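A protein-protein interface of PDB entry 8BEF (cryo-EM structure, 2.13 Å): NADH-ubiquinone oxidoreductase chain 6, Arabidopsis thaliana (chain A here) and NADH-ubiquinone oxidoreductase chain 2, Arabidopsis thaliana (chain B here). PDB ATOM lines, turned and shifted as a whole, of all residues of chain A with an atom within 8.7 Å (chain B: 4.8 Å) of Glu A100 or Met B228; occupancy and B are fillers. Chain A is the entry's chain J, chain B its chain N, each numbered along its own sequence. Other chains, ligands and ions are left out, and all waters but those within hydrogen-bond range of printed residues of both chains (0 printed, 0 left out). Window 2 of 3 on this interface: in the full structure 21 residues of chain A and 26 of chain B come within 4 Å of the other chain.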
ATOM      1  N   ILE A  93       2.245  40.407  -4.661  1.00  0.00           N
ATOM      2  CA  ILE A  93       1.489  39.665  -3.656  1.00  0.00           C
ATOM      3  C   ILE A  93       0.725  38.522  -4.310  1.00  0.00           C
ATOM      4  O   ILE A  93       0.699  37.398  -3.797  1.00  0.00           O
ATOM      5  CB  ILE A  93       0.550  40.605  -2.878  1.00  0.00           C
ATOM      6  CG1 ILE A  93       1.351  41.665  -2.118  1.00  0.00           C
ATOM      7  CG2 ILE A  93      -0.291  39.811  -1.902  1.00  0.00           C
ATOM      8  CD1 ILE A  93       2.099  41.140  -0.927  1.00  0.00           C
ATOM      9  N   GLY A  94       0.104  38.787  -5.460  1.00  0.00           N
ATOM     10  CA  GLY A  94      -0.598  37.729  -6.166  1.00  0.00           C
ATOM     11  C   GLY A  94       0.329  36.617  -6.619  1.00  0.00           C
ATOM     12  O   GLY A  94       0.046  35.437  -6.409  1.00  0.00           O
ATOM     13  N   LEU A  95       1.462  36.983  -7.227  1.00  0.00           N
ATOM     14  CA  LEU A  95       2.384  35.977  -7.753  1.00  0.00           C
ATOM     15  C   LEU A  95       2.951  35.103  -6.640  1.00  0.00           C
ATOM     16  O   LEU A  95       2.959  33.872  -6.751  1.00  0.00           O
ATOM     17  CB  LEU A  95       3.514  36.650  -8.529  1.00  0.00           C
ATOM     18  CG  LEU A  95       4.761  35.811  -8.808  1.00  0.00           C
ATOM     19  CD1 LEU A  95       4.536  34.900 -10.002  1.00  0.00           C
ATOM     20  CD2 LEU A  95       5.972  36.704  -9.030  1.00  0.00           C
ATOM     21  N   ILE A  96       3.433  35.722  -5.559  1.00  0.00           N
ATOM     22  CA  ILE A  96       3.947  34.953  -4.427  1.00  0.00           C
ATOM     23  C   ILE A  96       2.882  33.997  -3.914  1.00  0.00           C
ATOM     24  O   ILE A  96       3.133  32.801  -3.719  1.00  0.00           O
ATOM     25  CB  ILE A  96       4.438  35.888  -3.310  1.00  0.00           C
ATOM     26  CG1 ILE A  96       5.584  36.774  -3.802  1.00  0.00           C
ATOM     27  CG2 ILE A  96       4.823  35.090  -2.075  1.00  0.00           C
ATOM     28  CD1 ILE A  96       6.101  37.731  -2.753  1.00  0.00           C
ATOM     29  N   PHE A  97       1.674  34.511  -3.692  1.00  0.00           N
ATOM     30  CA  PHE A  97       0.568  33.642  -3.322  1.00  0.00           C
ATOM     31  C   PHE A  97       0.286  32.631  -4.424  1.00  0.00           C
ATOM     32  O   PHE A  97       0.034  31.457  -4.148  1.00  0.00           O
ATOM     33  CB  PHE A  97      -0.676  34.476  -3.019  1.00  0.00           C
ATOM     34  CG  PHE A  97      -0.790  34.897  -1.580  1.00  0.00           C
ATOM     35  CD1 PHE A  97      -0.203  36.074  -1.145  1.00  0.00           C
ATOM     36  CD2 PHE A  97      -1.486  34.126  -0.666  1.00  0.00           C
ATOM     37  CE1 PHE A  97      -0.305  36.475   0.175  1.00  0.00           C
ATOM     38  CE2 PHE A  97      -1.592  34.520   0.659  1.00  0.00           C
ATOM     39  CZ  PHE A  97      -0.998  35.697   1.078  1.00  0.00           C
ATOM     40  N   TRP A  98       0.349  33.061  -5.686  1.00  0.00           N
ATOM     41  CA  TRP A  98       0.121  32.123  -6.780  1.00  0.00           C
ATOM     42  C   TRP A  98       1.162  31.010  -6.789  1.00  0.00           C
ATOM     43  O   TRP A  98       0.813  29.825  -6.829  1.00  0.00           O
ATOM     44  CB  TRP A  98       0.127  32.854  -8.116  1.00  0.00           C
ATOM     45  CG  TRP A  98      -0.051  31.936  -9.276  1.00  0.00           C
ATOM     46  CD1 TRP A  98      -1.210  31.347  -9.692  1.00  0.00           C
ATOM     47  CD2 TRP A  98       0.974  31.471 -10.158  1.00  0.00           C
ATOM     48  NE1 TRP A  98      -0.972  30.560 -10.789  1.00  0.00           N
ATOM     49  CE2 TRP A  98       0.363  30.616 -11.094  1.00  0.00           C
ATOM     50  CE3 TRP A  98       2.350  31.698 -10.249  1.00  0.00           C
ATOM     51  CZ2 TRP A  98       1.079  29.989 -12.109  1.00  0.00           C
ATOM     52  CZ3 TRP A  98       3.059  31.074 -11.257  1.00  0.00           C
ATOM     53  CH2 TRP A  98       2.422  30.231 -12.174  1.00  0.00           C
ATOM     54  N   TRP A  99       2.446  31.372  -6.739  1.00  0.00           N
ATOM     55  CA  TRP A  99       3.514  30.380  -6.839  1.00  0.00           C
ATOM     56  C   TRP A  99       3.518  29.425  -5.656  1.00  0.00           C
ATOM     57  O   TRP A  99       3.869  28.249  -5.799  1.00  0.00           O
ATOM     58  CB  TRP A  99       4.868  31.079  -6.950  1.00  0.00           C
ATOM     59  CG  TRP A  99       6.030  30.144  -6.804  1.00  0.00           C
ATOM     60  CD1 TRP A  99       6.987  30.187  -5.836  1.00  0.00           C
ATOM     61  CD2 TRP A  99       6.347  29.016  -7.632  1.00  0.00           C
ATOM     62  NE1 TRP A  99       7.887  29.167  -6.013  1.00  0.00           N
ATOM     63  CE2 TRP A  99       7.517  28.432  -7.108  1.00  0.00           C
ATOM     64  CE3 TRP A  99       5.761  28.448  -8.768  1.00  0.00           C
ATOM     65  CZ2 TRP A  99       8.112  27.309  -7.678  1.00  0.00           C
ATOM     66  CZ3 TRP A  99       6.353  27.332  -9.332  1.00  0.00           C
ATOM     67  CH2 TRP A  99       7.516  26.775  -8.787  1.00  0.00           C
ATOM     68  N   GLU A 100       3.127  29.903  -4.487  1.00  0.00           N
ATOM     69  CA  GLU A 100       3.161  29.067  -3.301  1.00  0.00           C
ATOM     70  C   GLU A 100       1.903  28.238  -3.128  1.00  0.00           C
ATOM     71  O   GLU A 100       1.977  27.076  -2.722  1.00  0.00           O
ATOM     72  CB  GLU A 100       3.313  29.943  -2.064  1.00  0.00           C
ATOM     73  CG  GLU A 100       3.518  29.146  -0.833  1.00  0.00           C
ATOM     74  CD  GLU A 100       4.937  28.707  -0.718  1.00  0.00           C
ATOM     75  OE1 GLU A 100       5.825  29.556  -0.920  1.00  0.00           O
ATOM     76  OE2 GLU A 100       5.160  27.506  -0.467  1.00  0.00           O
ATOM     77  N   MET A 101       0.769  28.809  -3.439  1.00  0.00           N
ATOM     78  CA  MET A 101      -0.478  28.410  -2.825  1.00  0.00           C
ATOM     79  C   MET A 101      -1.426  27.711  -3.793  1.00  0.00           C
ATOM     80  O   MET A 101      -2.312  26.978  -3.351  1.00  0.00           O
ATOM     81  CB  MET A 101      -1.107  29.659  -2.184  1.00  0.00           C
ATOM     82  CG  MET A 101      -2.541  29.658  -1.989  1.00  0.00           C
ATOM     83  SD  MET A 101      -2.856  29.382  -0.233  1.00  0.00           S
ATOM     84  CE  MET A 101      -2.276  30.896   0.545  1.00  0.00           C
ATOM     85  N   PHE A 102      -1.260  27.912  -5.103  1.00  0.00           N
ATOM     86  CA  PHE A 102      -1.923  27.069  -6.098  1.00  0.00           C
ATOM     87  C   PHE A 102      -1.241  25.718  -6.267  1.00  0.00           C
ATOM     88  O   PHE A 102      -1.855  24.796  -6.806  1.00  0.00           O
ATOM     89  CB  PHE A 102      -1.969  27.766  -7.460  1.00  0.00           C
ATOM     90  CG  PHE A 102      -2.936  28.902  -7.536  1.00  0.00           C
ATOM     91  CD1 PHE A 102      -2.691  30.079  -6.849  1.00  0.00           C
ATOM     92  CD2 PHE A 102      -4.078  28.809  -8.309  1.00  0.00           C
ATOM     93  CE1 PHE A 102      -3.581  31.128  -6.922  1.00  0.00           C
ATOM     94  CE2 PHE A 102      -4.966  29.858  -8.387  1.00  0.00           C
ATOM     95  CZ  PHE A 102      -4.717  31.016  -7.694  1.00  0.00           C
ATOM     96  N   PHE A 103       0.009  25.587  -5.818  1.00  0.00           N
ATOM     97  CA  PHE A 103       0.807  24.383  -6.033  1.00  0.00           C
ATOM     98  C   PHE A 103       1.185  23.694  -4.731  1.00  0.00           C
ATOM     99  O   PHE A 103       2.065  22.827  -4.735  1.00  0.00           O
ATOM    100  CB  PHE A 103       2.071  24.726  -6.831  1.00  0.00           C
ATOM    101  CG  PHE A 103       1.799  25.518  -8.079  1.00  0.00           C
ATOM    102  CD1 PHE A 103       1.213  24.918  -9.180  1.00  0.00           C
ATOM    103  CD2 PHE A 103       2.108  26.867  -8.142  1.00  0.00           C
ATOM    104  CE1 PHE A 103       0.952  25.644 -10.329  1.00  0.00           C
ATOM    105  CE2 PHE A 103       1.848  27.597  -9.286  1.00  0.00           C
ATOM    106  CZ  PHE A 103       1.267  26.985 -10.380  1.00  0.00           C
ATOM    107  N   ILE A 104       0.543  24.057  -3.619  1.00  0.00           N
ATOM    108  CA  ILE A 104       0.899  23.507  -2.316  1.00  0.00           C
ATOM    109  C   ILE A 104       0.594  22.016  -2.246  1.00  0.00           C
ATOM    110  O   ILE A 104       1.316  21.258  -1.589  1.00  0.00           O
ATOM    111  CB  ILE A 104       0.179  24.305  -1.210  1.00  0.00           C
ATOM    112  CG1 ILE A 104       0.401  23.693   0.170  1.00  0.00           C
ATOM    113  CG2 ILE A 104      -1.284  24.401  -1.500  1.00  0.00           C
ATOM    114  CD1 ILE A 104       0.387  24.710   1.280  1.00  0.00           C
ATOM    115  N   LEU A 105      -0.465  21.569  -2.922  1.00  0.00           N
ATOM    116  CA  LEU A 105      -0.842  20.162  -2.912  1.00  0.00           C
ATOM    117  C   LEU A 105       0.003  19.304  -3.848  1.00  0.00           C
ATOM    118  O   LEU A 105      -0.067  18.074  -3.758  1.00  0.00           O
ATOM    119  CB  LEU A 105      -2.319  20.005  -3.294  1.00  0.00           C
ATOM    120  CG  LEU A 105      -3.398  20.716  -2.474  1.00  0.00           C
ATOM    121  CD1 LEU A 105      -4.761  20.088  -2.728  1.00  0.00           C
ATOM    122  CD2 LEU A 105      -3.075  20.690  -0.995  1.00  0.00           C
ATOM    123  N   ASP A 106       0.794  19.915  -4.734  1.00  0.00           N
ATOM    124  CA  ASP A 106       1.445  19.153  -5.797  1.00  0.00           C
ATOM    125  C   ASP A 106       2.438  18.133  -5.248  1.00  0.00           C
ATOM    126  O   ASP A 106       2.520  17.010  -5.755  1.00  0.00           O
ATOM    127  CB  ASP A 106       2.129  20.104  -6.777  1.00  0.00           C
ATOM    128  CG  ASP A 106       1.132  20.925  -7.575  1.00  0.00           C
ATOM    129  OD1 ASP A 106       0.073  21.280  -7.016  1.00  0.00           O
ATOM    130  OD2 ASP A 106       1.399  21.207  -8.760  1.00  0.00           O
ATOM    131  N   GLY B 193      -5.653  28.270   7.514  1.00  0.00           N
ATOM    132  CA  GLY B 193      -4.617  27.407   8.066  1.00  0.00           C
ATOM    133  C   GLY B 193      -5.171  26.098   8.595  1.00  0.00           C
ATOM    134  O   GLY B 193      -4.594  25.026   8.372  1.00  0.00           O
ATOM    135  N   SER B 224       4.314  20.803   2.836  1.00  0.00           N
ATOM    136  CA  SER B 224       4.093  22.236   2.707  1.00  0.00           C
ATOM    137  C   SER B 224       2.688  22.623   3.157  1.00  0.00           C
ATOM    138  O   SER B 224       2.479  23.737   3.656  1.00  0.00           O
ATOM    139  CB  SER B 224       4.372  22.655   1.264  1.00  0.00           C
ATOM    140  OG  SER B 224       3.196  22.696   0.493  1.00  0.00           O
ATOM    141  N   GLY B 225       1.728  21.704   3.028  1.00  0.00           N
ATOM    142  CA  GLY B 225       0.389  21.967   3.530  1.00  0.00           C
ATOM    143  C   GLY B 225       0.349  22.157   5.035  1.00  0.00           C
ATOM    144  O   GLY B 225      -0.222  23.130   5.532  1.00  0.00           O
ATOM    145  N   ILE B 226       1.008  21.233   5.736  1.00  0.00           N
ATOM    146  CA  ILE B 226       1.191  21.331   7.207  1.00  0.00           C
ATOM    147  C   ILE B 226       1.981  22.593   7.572  1.00  0.00           C
ATOM    148  O   ILE B 226       1.508  23.316   8.449  1.00  0.00           O
ATOM    149  CB  ILE B 226       1.865  20.077   7.772  1.00  0.00           C
ATOM    150  CG1 ILE B 226       1.027  18.819   7.548  1.00  0.00           C
ATOM    151  CG2 ILE B 226       2.192  20.256   9.249  1.00  0.00           C
ATOM    152  CD1 ILE B 226       1.746  17.549   7.931  1.00  0.00           C
ATOM    153  N   PHE B 227       3.048  22.900   6.853  1.00  0.00           N
ATOM    154  CA  PHE B 227       3.874  24.072   7.202  1.00  0.00           C
ATOM    155  C   PHE B 227       3.058  25.383   7.038  1.00  0.00           C
ATOM    156  O   PHE B 227       3.130  26.195   7.942  1.00  0.00           O
ATOM    157  CB  PHE B 227       5.192  24.052   6.428  1.00  0.00           C
ATOM    158  CG  PHE B 227       6.168  25.108   6.827  1.00  0.00           C
ATOM    159  CD1 PHE B 227       6.061  26.386   6.316  1.00  0.00           C
ATOM    160  CD2 PHE B 227       7.168  24.816   7.736  1.00  0.00           C
ATOM    161  CE1 PHE B 227       6.965  27.358   6.694  1.00  0.00           C
ATOM    162  CE2 PHE B 227       8.070  25.790   8.104  1.00  0.00           C
ATOM    163  CZ  PHE B 227       7.963  27.057   7.587  1.00  0.00           C
ATOM    164  N   MET B 228       2.290  25.546   5.973  1.00  0.00           N
ATOM    165  CA  MET B 228       1.535  26.782   5.780  1.00  0.00           C
ATOM    166  C   MET B 228       0.267  26.831   6.619  1.00  0.00           C
ATOM    167  O   MET B 228      -0.168  27.920   7.014  1.00  0.00           O
ATOM    168  CB  MET B 228       1.246  27.001   4.301  1.00  0.00           C
ATOM    169  CG  MET B 228       2.526  26.973   3.546  1.00  0.00           C
ATOM    170  SD  MET B 228       2.868  28.662   3.057  1.00  0.00           S
ATOM    171  CE  MET B 228       4.524  28.451   2.458  1.00  0.00           C
ATOM    172  N   GLY B 229      -0.341  25.682   6.918  1.00  0.00           N
ATOM    173  CA  GLY B 229      -1.437  25.689   7.873  1.00  0.00           C
ATOM    174  C   GLY B 229      -0.995  26.219   9.223  1.00  0.00           C
ATOM    175  O   GLY B 229      -1.659  27.072   9.825  1.00  0.00           O
ATOM    176  N   ILE B 230       0.129  25.708   9.713  1.00  0.00           N
ATOM    177  CA  ILE B 230       0.745  26.239  10.963  1.00  0.00           C
ATOM    178  C   ILE B 230       0.994  27.750  10.813  1.00  0.00           C
ATOM    179  O   ILE B 230       0.698  28.458  11.700  1.00  0.00           O
ATOM    180  CB  ILE B 230       2.068  25.496  11.343  1.00  0.00           C
ATOM    181  CG1 ILE B 230       1.837  24.004  11.554  1.00  0.00           C
ATOM    182  CG2 ILE B 230       2.761  26.139  12.529  1.00  0.00           C
ATOM    183  CD1 ILE B 230       0.759  23.726  12.533  1.00  0.00           C
ATOM    184  N   LEU B 231       1.563  28.184   9.721  1.00  0.00           N
ATOM    185  CA  LEU B 231       1.873  29.605   9.586  1.00  0.00           C
ATOM    186  C   LEU B 231       0.616  30.466   9.674  1.00  0.00           C
ATOM    187  O   LEU B 231       0.594  31.483  10.379  1.00  0.00           O
ATOM    188  CB  LEU B 231       2.593  29.874   8.269  1.00  0.00           C
ATOM    189  CG  LEU B 231       4.100  29.697   8.343  1.00  0.00           C
ATOM    190  CD1 LEU B 231       4.690  29.752   6.946  1.00  0.00           C
ATOM    191  CD2 LEU B 231       4.707  30.722   9.276  1.00  0.00           C
ATOM    192  N   PHE B 232      -0.440  30.079   8.955  1.00  0.00           N
ATOM    193  CA  PHE B 232      -1.667  30.873   8.958  1.00  0.00           C
ATOM    194  C   PHE B 232      -2.319  30.878  10.339  1.00  0.00           C
ATOM    195  O   PHE B 232      -2.808  31.922  10.805  1.00  0.00           O
ATOM    196  CB  PHE B 232      -2.631  30.344   7.892  1.00  0.00           C
ATOM    197  CG  PHE B 232      -2.348  30.859   6.499  1.00  0.00           C
ATOM    198  CD1 PHE B 232      -1.102  30.690   5.917  1.00  0.00           C
ATOM    199  CD2 PHE B 232      -3.333  31.507   5.773  1.00  0.00           C
ATOM    200  CE1 PHE B 232      -0.841  31.157   4.640  1.00  0.00           C
ATOM    201  CE2 PHE B 232      -3.078  31.979   4.492  1.00  0.00           C
ATOM    202  CZ  PHE B 232      -1.831  31.801   3.927  1.00  0.00           C
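O of Ile A104 lies close to OG of Ser B224 (3.2 Å).
Glu A100 touches Met B228.
CE of Met A101 touches CZ of Phe B232 (3.5 Å).
Ile A104 touches Gly B225.
Met B228 touches Ile A104.
Glu A100 touches just one residue of chain B: Met B228.
Printed residues of chain B within 4 Å of Met A101: Phe B232 (3.5 Å).
Printed residues of chain A within 4 Å of Gly B225: Ile A104.
Of the printed residues of chain A, Met B228 touches Glu A100 (3.1 Å) and Ile A104 (3.9 Å).
Of the printed residues of chain A, Phe B232 touches Met A101 (3.5 Å).
The nearest printed residue of chain B that does not touch Glu A100 is Ser B224 (5.2 Å).
Of the 10 printed residues of chain B, 4 touch a printed residue of chain A.
Hydrophobic or aromatic side chains of chain B that line the printed part of chain A: Met B228 and Phe B232.
Of the 14 printed residues of chain A, 3 touch a printed residue of chain B.
Hydrophobic or aromatic side chains of chain A that line the printed part of chain B: Met A101 and Ile A104.
Among the printed residues, no Asp or Glu carboxylate lies within 4 Å of a Lys or Arg side-chain nitrogen of the other chain.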
